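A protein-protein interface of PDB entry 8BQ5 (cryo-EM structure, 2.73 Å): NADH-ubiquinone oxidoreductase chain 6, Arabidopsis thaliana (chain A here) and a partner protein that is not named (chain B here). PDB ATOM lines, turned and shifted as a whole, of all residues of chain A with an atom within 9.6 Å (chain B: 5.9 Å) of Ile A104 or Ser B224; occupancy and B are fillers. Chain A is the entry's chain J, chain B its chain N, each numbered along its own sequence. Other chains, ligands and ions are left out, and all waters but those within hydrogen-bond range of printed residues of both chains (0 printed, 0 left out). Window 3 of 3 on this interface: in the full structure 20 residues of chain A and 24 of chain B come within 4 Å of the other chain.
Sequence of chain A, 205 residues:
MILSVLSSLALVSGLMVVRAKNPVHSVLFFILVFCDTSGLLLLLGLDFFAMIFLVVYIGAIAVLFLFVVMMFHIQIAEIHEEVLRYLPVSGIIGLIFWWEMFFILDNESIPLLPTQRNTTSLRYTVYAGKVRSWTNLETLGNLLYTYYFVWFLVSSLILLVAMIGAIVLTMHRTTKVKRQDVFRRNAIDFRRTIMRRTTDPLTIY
O of Ile A104 sits close to OG of Ser B224 (3.1 Å).
OE2 of Glu A108 sits at hydrogen-bond distance from OG of Ser B223.
Among the printed residues, merely in contact across the chains: Glu A100 with Met B228, Ile A104 with Met B196, Ile A104 with Gly B225 and Leu A105 with Met B196.
Of chain B, only Met B196, Ser B224 and Gly B225 come within 4 Å of Ile A104.
Of chain A, only Ile A104 (3.1 Å) comes within 4 Å of Ser B224.
Gly B225 touches just one residue of chain A: Ile A104.
Of the printed residues of chain B, Leu A105 touches Met B196.
Printed residues of chain B within 4 Å of Glu A108: Ser B223.
The nearest residue of chain A that does not touch Ser B224 is Glu A108 (5.0 Å).
Hydrophobic or aromatic side chains of chain A within 4 Å of the printed part of chain B: Ile A104 and Leu A105.
Printed residues of chain B that touch a printed residue of chain A: Met B196, Ser B223, Ser B224, Gly B225 and Met B228.
Hydrophobic or aromatic side chains of chain B that line the printed part of chain A: Met B196 and Met B228.
Among the printed residues, 6 pairs touch across the chains.
Among the printed residues, no Asp or Glu carboxylate lies within 4 Å of a Lys or Arg side-chain nitrogen of the other chain.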
ATOM      1  N   ILE A  96      24.846 -14.693   1.876  1.00  0.00           N
ATOM      2  CA  ILE A  96      24.584 -13.342   1.384  1.00  0.00           C
ATOM      3  C   ILE A  96      23.424 -13.355   0.399  1.00  0.00           C
ATOM      4  O   ILE A  96      22.460 -12.587   0.530  1.00  0.00           O
ATOM      5  CB  ILE A  96      25.853 -12.745   0.750  1.00  0.00           C
ATOM      6  CG1 ILE A  96      26.956 -12.603   1.803  1.00  0.00           C
ATOM      7  CG2 ILE A  96      25.546 -11.423   0.063  1.00  0.00           C
ATOM      8  CD1 ILE A  96      28.156 -11.810   1.336  1.00  0.00           C
ATOM      9  N   PHE A  97      23.493 -14.247  -0.593  1.00  0.00           N
ATOM     10  CA  PHE A  97      22.434 -14.333  -1.589  1.00  0.00           C
ATOM     11  C   PHE A  97      21.108 -14.707  -0.944  1.00  0.00           C
ATOM     12  O   PHE A  97      20.064 -14.157  -1.298  1.00  0.00           O
ATOM     13  CB  PHE A  97      22.813 -15.345  -2.666  1.00  0.00           C
ATOM     14  CG  PHE A  97      23.476 -14.737  -3.862  1.00  0.00           C
ATOM     15  CD1 PHE A  97      24.854 -14.631  -3.924  1.00  0.00           C
ATOM     16  CD2 PHE A  97      22.724 -14.262  -4.921  1.00  0.00           C
ATOM     17  CE1 PHE A  97      25.471 -14.071  -5.024  1.00  0.00           C
ATOM     18  CE2 PHE A  97      23.334 -13.699  -6.024  1.00  0.00           C
ATOM     19  CZ  PHE A  97      24.709 -13.603  -6.074  1.00  0.00           C
ATOM     20  N   TRP A  98      21.136 -15.626   0.020  1.00  0.00           N
ATOM     21  CA  TRP A  98      19.920 -16.056   0.693  1.00  0.00           C
ATOM     22  C   TRP A  98      19.244 -14.897   1.406  1.00  0.00           C
ATOM     23  O   TRP A  98      18.070 -14.601   1.154  1.00  0.00           O
ATOM     24  CB  TRP A  98      20.252 -17.179   1.675  1.00  0.00           C
ATOM     25  CG  TRP A  98      19.132 -17.530   2.597  1.00  0.00           C
ATOM     26  CD1 TRP A  98      18.050 -18.310   2.318  1.00  0.00           C
ATOM     27  CD2 TRP A  98      18.983 -17.103   3.954  1.00  0.00           C
ATOM     28  NE1 TRP A  98      17.236 -18.400   3.423  1.00  0.00           N
ATOM     29  CE2 TRP A  98      17.788 -17.666   4.440  1.00  0.00           C
ATOM     30  CE3 TRP A  98      19.746 -16.300   4.807  1.00  0.00           C
ATOM     31  CZ2 TRP A  98      17.339 -17.449   5.740  1.00  0.00           C
ATOM     32  CZ3 TRP A  98      19.299 -16.088   6.094  1.00  0.00           C
ATOM     33  CH2 TRP A  98      18.106 -16.661   6.550  1.00  0.00           C
ATOM     34  N   TRP A  99      19.981 -14.204   2.275  1.00  0.00           N
ATOM     35  CA  TRP A  99      19.365 -13.131   3.045  1.00  0.00           C
ATOM     36  C   TRP A  99      18.916 -11.988   2.145  1.00  0.00           C
ATOM     37  O   TRP A  99      17.830 -11.434   2.351  1.00  0.00           O
ATOM     38  CB  TRP A  99      20.327 -12.669   4.150  1.00  0.00           C
ATOM     39  CG  TRP A  99      20.242 -11.220   4.594  1.00  0.00           C
ATOM     40  CD1 TRP A  99      19.122 -10.443   4.695  1.00  0.00           C
ATOM     41  CD2 TRP A  99      21.321 -10.423   5.101  1.00  0.00           C
ATOM     42  NE1 TRP A  99      19.447  -9.198   5.168  1.00  0.00           N
ATOM     43  CE2 TRP A  99      20.789  -9.162   5.436  1.00  0.00           C
ATOM     44  CE3 TRP A  99      22.688 -10.647   5.285  1.00  0.00           C
ATOM     45  CZ2 TRP A  99      21.576  -8.130   5.941  1.00  0.00           C
ATOM     46  CZ3 TRP A  99      23.466  -9.623   5.787  1.00  0.00           C
ATOM     47  CH2 TRP A  99      22.910  -8.380   6.107  1.00  0.00           C
ATOM     48  N   GLU A 100      19.700 -11.635   1.129  1.00  0.00           N
ATOM     49  CA  GLU A 100      19.281 -10.513   0.303  1.00  0.00           C
ATOM     50  C   GLU A 100      18.163 -10.883  -0.668  1.00  0.00           C
ATOM     51  O   GLU A 100      17.366 -10.017  -1.047  1.00  0.00           O
ATOM     52  CB  GLU A 100      20.482  -9.952  -0.465  1.00  0.00           C
ATOM     53  CG  GLU A 100      20.178  -8.698  -1.264  1.00  0.00           C
ATOM     54  CD  GLU A 100      20.054  -7.469  -0.380  1.00  0.00           C
ATOM     55  OE1 GLU A 100      20.942  -7.252   0.470  1.00  0.00           O
ATOM     56  OE2 GLU A 100      19.067  -6.718  -0.535  1.00  0.00           O
ATOM     57  N   MET A 101      18.042 -12.160  -1.044  1.00  0.00           N
ATOM     58  CA  MET A 101      17.312 -12.514  -2.247  1.00  0.00           C
ATOM     59  C   MET A 101      16.111 -13.425  -2.019  1.00  0.00           C
ATOM     60  O   MET A 101      15.178 -13.389  -2.825  1.00  0.00           O
ATOM     61  CB  MET A 101      18.284 -13.173  -3.237  1.00  0.00           C
ATOM     62  CG  MET A 101      17.915 -12.993  -4.676  1.00  0.00           C
ATOM     63  SD  MET A 101      18.192 -11.339  -5.326  1.00  0.00           S
ATOM     64  CE  MET A 101      19.707 -10.898  -4.489  1.00  0.00           C
ATOM     65  N   PHE A 102      16.102 -14.238  -0.957  1.00  0.00           N
ATOM     66  CA  PHE A 102      14.892 -14.974  -0.602  1.00  0.00           C
ATOM     67  C   PHE A 102      13.843 -14.102   0.073  1.00  0.00           C
ATOM     68  O   PHE A 102      12.686 -14.522   0.180  1.00  0.00           O
ATOM     69  CB  PHE A 102      15.219 -16.163   0.309  1.00  0.00           C
ATOM     70  CG  PHE A 102      15.946 -17.283  -0.376  1.00  0.00           C
ATOM     71  CD1 PHE A 102      15.325 -18.505  -0.561  1.00  0.00           C
ATOM     72  CD2 PHE A 102      17.234 -17.122  -0.843  1.00  0.00           C
ATOM     73  CE1 PHE A 102      15.979 -19.544  -1.188  1.00  0.00           C
ATOM     74  CE2 PHE A 102      17.897 -18.158  -1.469  1.00  0.00           C
ATOM     75  CZ  PHE A 102      17.267 -19.370  -1.644  1.00  0.00           C
ATOM     76  N   PHE A 103      14.216 -12.910   0.536  1.00  0.00           N
ATOM     77  CA  PHE A 103      13.273 -11.990   1.157  1.00  0.00           C
ATOM     78  C   PHE A 103      13.133 -10.694   0.370  1.00  0.00           C
ATOM     79  O   PHE A 103      12.858  -9.644   0.964  1.00  0.00           O
ATOM     80  CB  PHE A 103      13.692 -11.702   2.602  1.00  0.00           C
ATOM     81  CG  PHE A 103      14.147 -12.925   3.346  1.00  0.00           C
ATOM     82  CD1 PHE A 103      13.230 -13.865   3.786  1.00  0.00           C
ATOM     83  CD2 PHE A 103      15.491 -13.145   3.587  1.00  0.00           C
ATOM     84  CE1 PHE A 103      13.646 -14.997   4.461  1.00  0.00           C
ATOM     85  CE2 PHE A 103      15.912 -14.274   4.260  1.00  0.00           C
ATOM     86  CZ  PHE A 103      14.987 -15.201   4.696  1.00  0.00           C
ATOM     87  N   ILE A 104      13.308 -10.744  -0.951  1.00  0.00           N
ATOM     88  CA  ILE A 104      13.241  -9.531  -1.756  1.00  0.00           C
ATOM     89  C   ILE A 104      11.797  -9.094  -1.955  1.00  0.00           C
ATOM     90  O   ILE A 104      11.526  -7.908  -2.175  1.00  0.00           O
ATOM     91  CB  ILE A 104      13.972  -9.757  -3.091  1.00  0.00           C
ATOM     92  CG1 ILE A 104      14.146  -8.451  -3.855  1.00  0.00           C
ATOM     93  CG2 ILE A 104      13.169 -10.678  -3.953  1.00  0.00           C
ATOM     94  CD1 ILE A 104      14.594  -8.647  -5.249  1.00  0.00           C
ATOM     95  N   LEU A 105      10.850 -10.028  -1.874  1.00  0.00           N
ATOM     96  CA  LEU A 105       9.444  -9.691  -2.035  1.00  0.00           C
ATOM     97  C   LEU A 105       8.751  -9.374  -0.716  1.00  0.00           C
ATOM     98  O   LEU A 105       7.616  -8.893  -0.740  1.00  0.00           O
ATOM     99  CB  LEU A 105       8.700 -10.835  -2.735  1.00  0.00           C
ATOM    100  CG  LEU A 105       9.184 -11.296  -4.113  1.00  0.00           C
ATOM    101  CD1 LEU A 105       8.130 -12.160  -4.787  1.00  0.00           C
ATOM    102  CD2 LEU A 105       9.534 -10.108  -4.990  1.00  0.00           C
ATOM    103  N   ASP A 106       9.404  -9.612   0.425  1.00  0.00           N
ATOM    104  CA  ASP A 106       8.715  -9.491   1.707  1.00  0.00           C
ATOM    105  C   ASP A 106       8.279  -8.056   1.981  1.00  0.00           C
ATOM    106  O   ASP A 106       7.158  -7.820   2.447  1.00  0.00           O
ATOM    107  CB  ASP A 106       9.608 -10.015   2.830  1.00  0.00           C
ATOM    108  CG  ASP A 106       9.771 -11.522   2.781  1.00  0.00           C
ATOM    109  OD1 ASP A 106       9.962 -12.058   1.670  1.00  0.00           O
ATOM    110  OD2 ASP A 106       9.707 -12.170   3.846  1.00  0.00           O
ATOM    111  N   ASN A 107       9.145  -7.084   1.698  1.00  0.00           N
ATOM    112  CA  ASN A 107       8.776  -5.689   1.906  1.00  0.00           C
ATOM    113  C   ASN A 107       7.763  -5.206   0.877  1.00  0.00           C
ATOM    114  O   ASN A 107       6.869  -4.422   1.214  1.00  0.00           O
ATOM    115  CB  ASN A 107      10.021  -4.803   1.874  1.00  0.00           C
ATOM    116  CG  ASN A 107      10.897  -4.990   3.093  1.00  0.00           C
ATOM    117  OD1 ASN A 107      10.431  -5.429   4.145  1.00  0.00           O
ATOM    118  ND2 ASN A 107      12.177  -4.660   2.961  1.00  0.00           N
ATOM    119  N   GLU A 108       7.886  -5.655  -0.372  1.00  0.00           N
ATOM    120  CA  GLU A 108       6.938  -5.254  -1.405  1.00  0.00           C
ATOM    121  C   GLU A 108       5.654  -6.069  -1.336  1.00  0.00           C
ATOM    122  O   GLU A 108       4.558  -5.519  -1.483  1.00  0.00           O
ATOM    123  CB  GLU A 108       7.587  -5.392  -2.781  1.00  0.00           C
ATOM    124  CG  GLU A 108       6.762  -4.841  -3.922  1.00  0.00           C
ATOM    125  CD  GLU A 108       7.624  -4.364  -5.072  1.00  0.00           C
ATOM    126  OE1 GLU A 108       7.089  -3.705  -5.987  1.00  0.00           O
ATOM    127  OE2 GLU A 108       8.840  -4.648  -5.057  1.00  0.00           O
ATOM    128  N   SER A 109       5.767  -7.372  -1.110  1.00  0.00           N
ATOM    129  CA  SER A 109       4.616  -8.270  -1.042  1.00  0.00           C
ATOM    130  C   SER A 109       4.568  -8.852   0.366  1.00  0.00           C
ATOM    131  O   SER A 109       5.091  -9.937   0.628  1.00  0.00           O
ATOM    132  CB  SER A 109       4.715  -9.361  -2.098  1.00  0.00           C
ATOM    133  OG  SER A 109       4.202  -8.911  -3.338  1.00  0.00           O
ATOM    134  N   ILE A 110       3.934  -8.121   1.269  1.00  0.00           N
ATOM    135  CA  ILE A 110       3.798  -8.573   2.654  1.00  0.00           C
ATOM    136  C   ILE A 110       2.763  -9.693   2.705  1.00  0.00           C
ATOM    137  O   ILE A 110       1.636  -9.504   2.223  1.00  0.00           O
ATOM    138  CB  ILE A 110       3.405  -7.410   3.553  1.00  0.00           C
ATOM    139  CG1 ILE A 110       4.435  -6.295   3.402  1.00  0.00           C
ATOM    140  CG2 ILE A 110       3.323  -7.851   5.007  1.00  0.00           C
ATOM    141  CD1 ILE A 110       4.046  -5.028   4.069  1.00  0.00           C
ATOM    142  N   MET B 196      12.988  -9.507 -12.203  1.00  0.00           N
ATOM    143  CA  MET B 196      12.761  -8.774 -10.962  1.00  0.00           C
ATOM    144  C   MET B 196      12.053  -7.449 -11.230  1.00  0.00           C
ATOM    145  O   MET B 196      11.111  -7.076 -10.514  1.00  0.00           O
ATOM    146  CB  MET B 196      14.083  -8.528 -10.236  1.00  0.00           C
ATOM    147  CG  MET B 196      14.579  -9.683  -9.373  1.00  0.00           C
ATOM    148  SD  MET B 196      13.255 -10.715  -8.716  1.00  0.00           S
ATOM    149  CE  MET B 196      12.553  -9.653  -7.484  1.00  0.00           C
ATOM    150  N   ARG B 222      12.066   2.040  -0.388  1.00  0.00           N
ATOM    151  CA  ARG B 222      12.635   1.706  -1.685  1.00  0.00           C
ATOM    152  C   ARG B 222      12.309   0.268  -2.068  1.00  0.00           C
ATOM    153  O   ARG B 222      12.533  -0.662  -1.289  1.00  0.00           O
ATOM    154  CB  ARG B 222      14.151   1.903  -1.671  1.00  0.00           C
ATOM    155  CG  ARG B 222      14.857   1.219  -2.825  1.00  0.00           C
ATOM    156  CD  ARG B 222      16.364   1.188  -2.661  1.00  0.00           C
ATOM    157  NE  ARG B 222      16.783   0.124  -1.757  1.00  0.00           N
ATOM    158  CZ  ARG B 222      18.018  -0.028  -1.299  1.00  0.00           C
ATOM    159  NH1 ARG B 222      19.002   0.768  -1.683  1.00  0.00           N
ATOM    160  NH2 ARG B 222      18.275  -1.012  -0.442  1.00  0.00           N
ATOM    161  N   SER B 223      11.785   0.096  -3.278  1.00  0.00           N
ATOM    162  CA  SER B 223      11.507  -1.232  -3.817  1.00  0.00           C
ATOM    163  C   SER B 223      12.829  -1.955  -4.018  1.00  0.00           C
ATOM    164  O   SER B 223      13.603  -1.626  -4.919  1.00  0.00           O
ATOM    165  CB  SER B 223      10.730  -1.130  -5.125  1.00  0.00           C
ATOM    166  OG  SER B 223      10.408  -2.416  -5.628  1.00  0.00           O
ATOM    167  N   SER B 224      13.102  -2.939  -3.162  1.00  0.00           N
ATOM    168  CA  SER B 224      14.339  -3.698  -3.287  1.00  0.00           C
ATOM    169  C   SER B 224      14.355  -4.527  -4.567  1.00  0.00           C
ATOM    170  O   SER B 224      15.428  -4.797  -5.122  1.00  0.00           O
ATOM    171  CB  SER B 224      14.526  -4.577  -2.053  1.00  0.00           C
ATOM    172  OG  SER B 224      13.888  -5.828  -2.212  1.00  0.00           O
ATOM    173  N   GLY B 225      13.174  -4.913  -5.058  1.00  0.00           N
ATOM    174  CA  GLY B 225      13.105  -5.634  -6.319  1.00  0.00           C
ATOM    175  C   GLY B 225      13.581  -4.802  -7.494  1.00  0.00           C
ATOM    176  O   GLY B 225      14.325  -5.284  -8.349  1.00  0.00           O
ATOM    177  N   ILE B 226      13.160  -3.537  -7.550  1.00  0.00           N
ATOM    178  CA  ILE B 226      13.613  -2.658  -8.624  1.00  0.00           C
ATOM    179  C   ILE B 226      15.115  -2.419  -8.519  1.00  0.00           C
ATOM    180  O   ILE B 226      15.832  -2.429  -9.528  1.00  0.00           O
ATOM    181  CB  ILE B 226      12.826  -1.336  -8.608  1.00  0.00           C
ATOM    182  CG1 ILE B 226      11.340  -1.599  -8.826  1.00  0.00           C
ATOM    183  CG2 ILE B 226      13.325  -0.414  -9.697  1.00  0.00           C
ATOM    184  CD1 ILE B 226      10.480  -0.366  -8.692  1.00  0.00           C
ATOM    185  N   PHE B 227      15.612  -2.198  -7.297  1.00  0.00           N
ATOM    186  CA  PHE B 227      17.048  -2.031  -7.091  1.00  0.00           C
ATOM    187  C   PHE B 227      17.840  -3.214  -7.627  1.00  0.00           C
ATOM    188  O   PHE B 227      18.774  -3.036  -8.417  1.00  0.00           O
ATOM    189  CB  PHE B 227      17.350  -1.841  -5.606  1.00  0.00           C
ATOM    190  CG  PHE B 227      18.528  -0.955  -5.334  1.00  0.00           C
ATOM    191  CD1 PHE B 227      18.411   0.416  -5.375  1.00  0.00           C
ATOM    192  CD2 PHE B 227      19.763  -1.504  -5.046  1.00  0.00           C
ATOM    193  CE1 PHE B 227      19.495   1.231  -5.128  1.00  0.00           C
ATOM    194  CE2 PHE B 227      20.851  -0.699  -4.798  1.00  0.00           C
ATOM    195  CZ  PHE B 227      20.716   0.673  -4.837  1.00  0.00           C
ATOM    196  N   MET B 228      17.488  -4.430  -7.207  1.00  0.00           N
ATOM    197  CA  MET B 228      18.247  -5.590  -7.661  1.00  0.00           C
ATOM    198  C   MET B 228      18.036  -5.895  -9.137  1.00  0.00           C
ATOM    199  O   MET B 228      18.957  -6.398  -9.790  1.00  0.00           O
ATOM    200  CB  MET B 228      17.921  -6.808  -6.800  1.00  0.00           C
ATOM    201  CG  MET B 228      18.108  -6.538  -5.328  1.00  0.00           C
ATOM    202  SD  MET B 228      19.831  -6.861  -4.911  1.00  0.00           S
ATOM    203  CE  MET B 228      20.017  -5.899  -3.421  1.00  0.00           C
ATOM    204  N   GLY B 229      16.859  -5.599  -9.690  1.00  0.00           N
ATOM    205  CA  GLY B 229      16.694  -5.729 -11.126  1.00  0.00           C
ATOM    206  C   GLY B 229      17.646  -4.827 -11.885  1.00  0.00           C
ATOM    207  O   GLY B 229      18.324  -5.260 -12.824  1.00  0.00           O
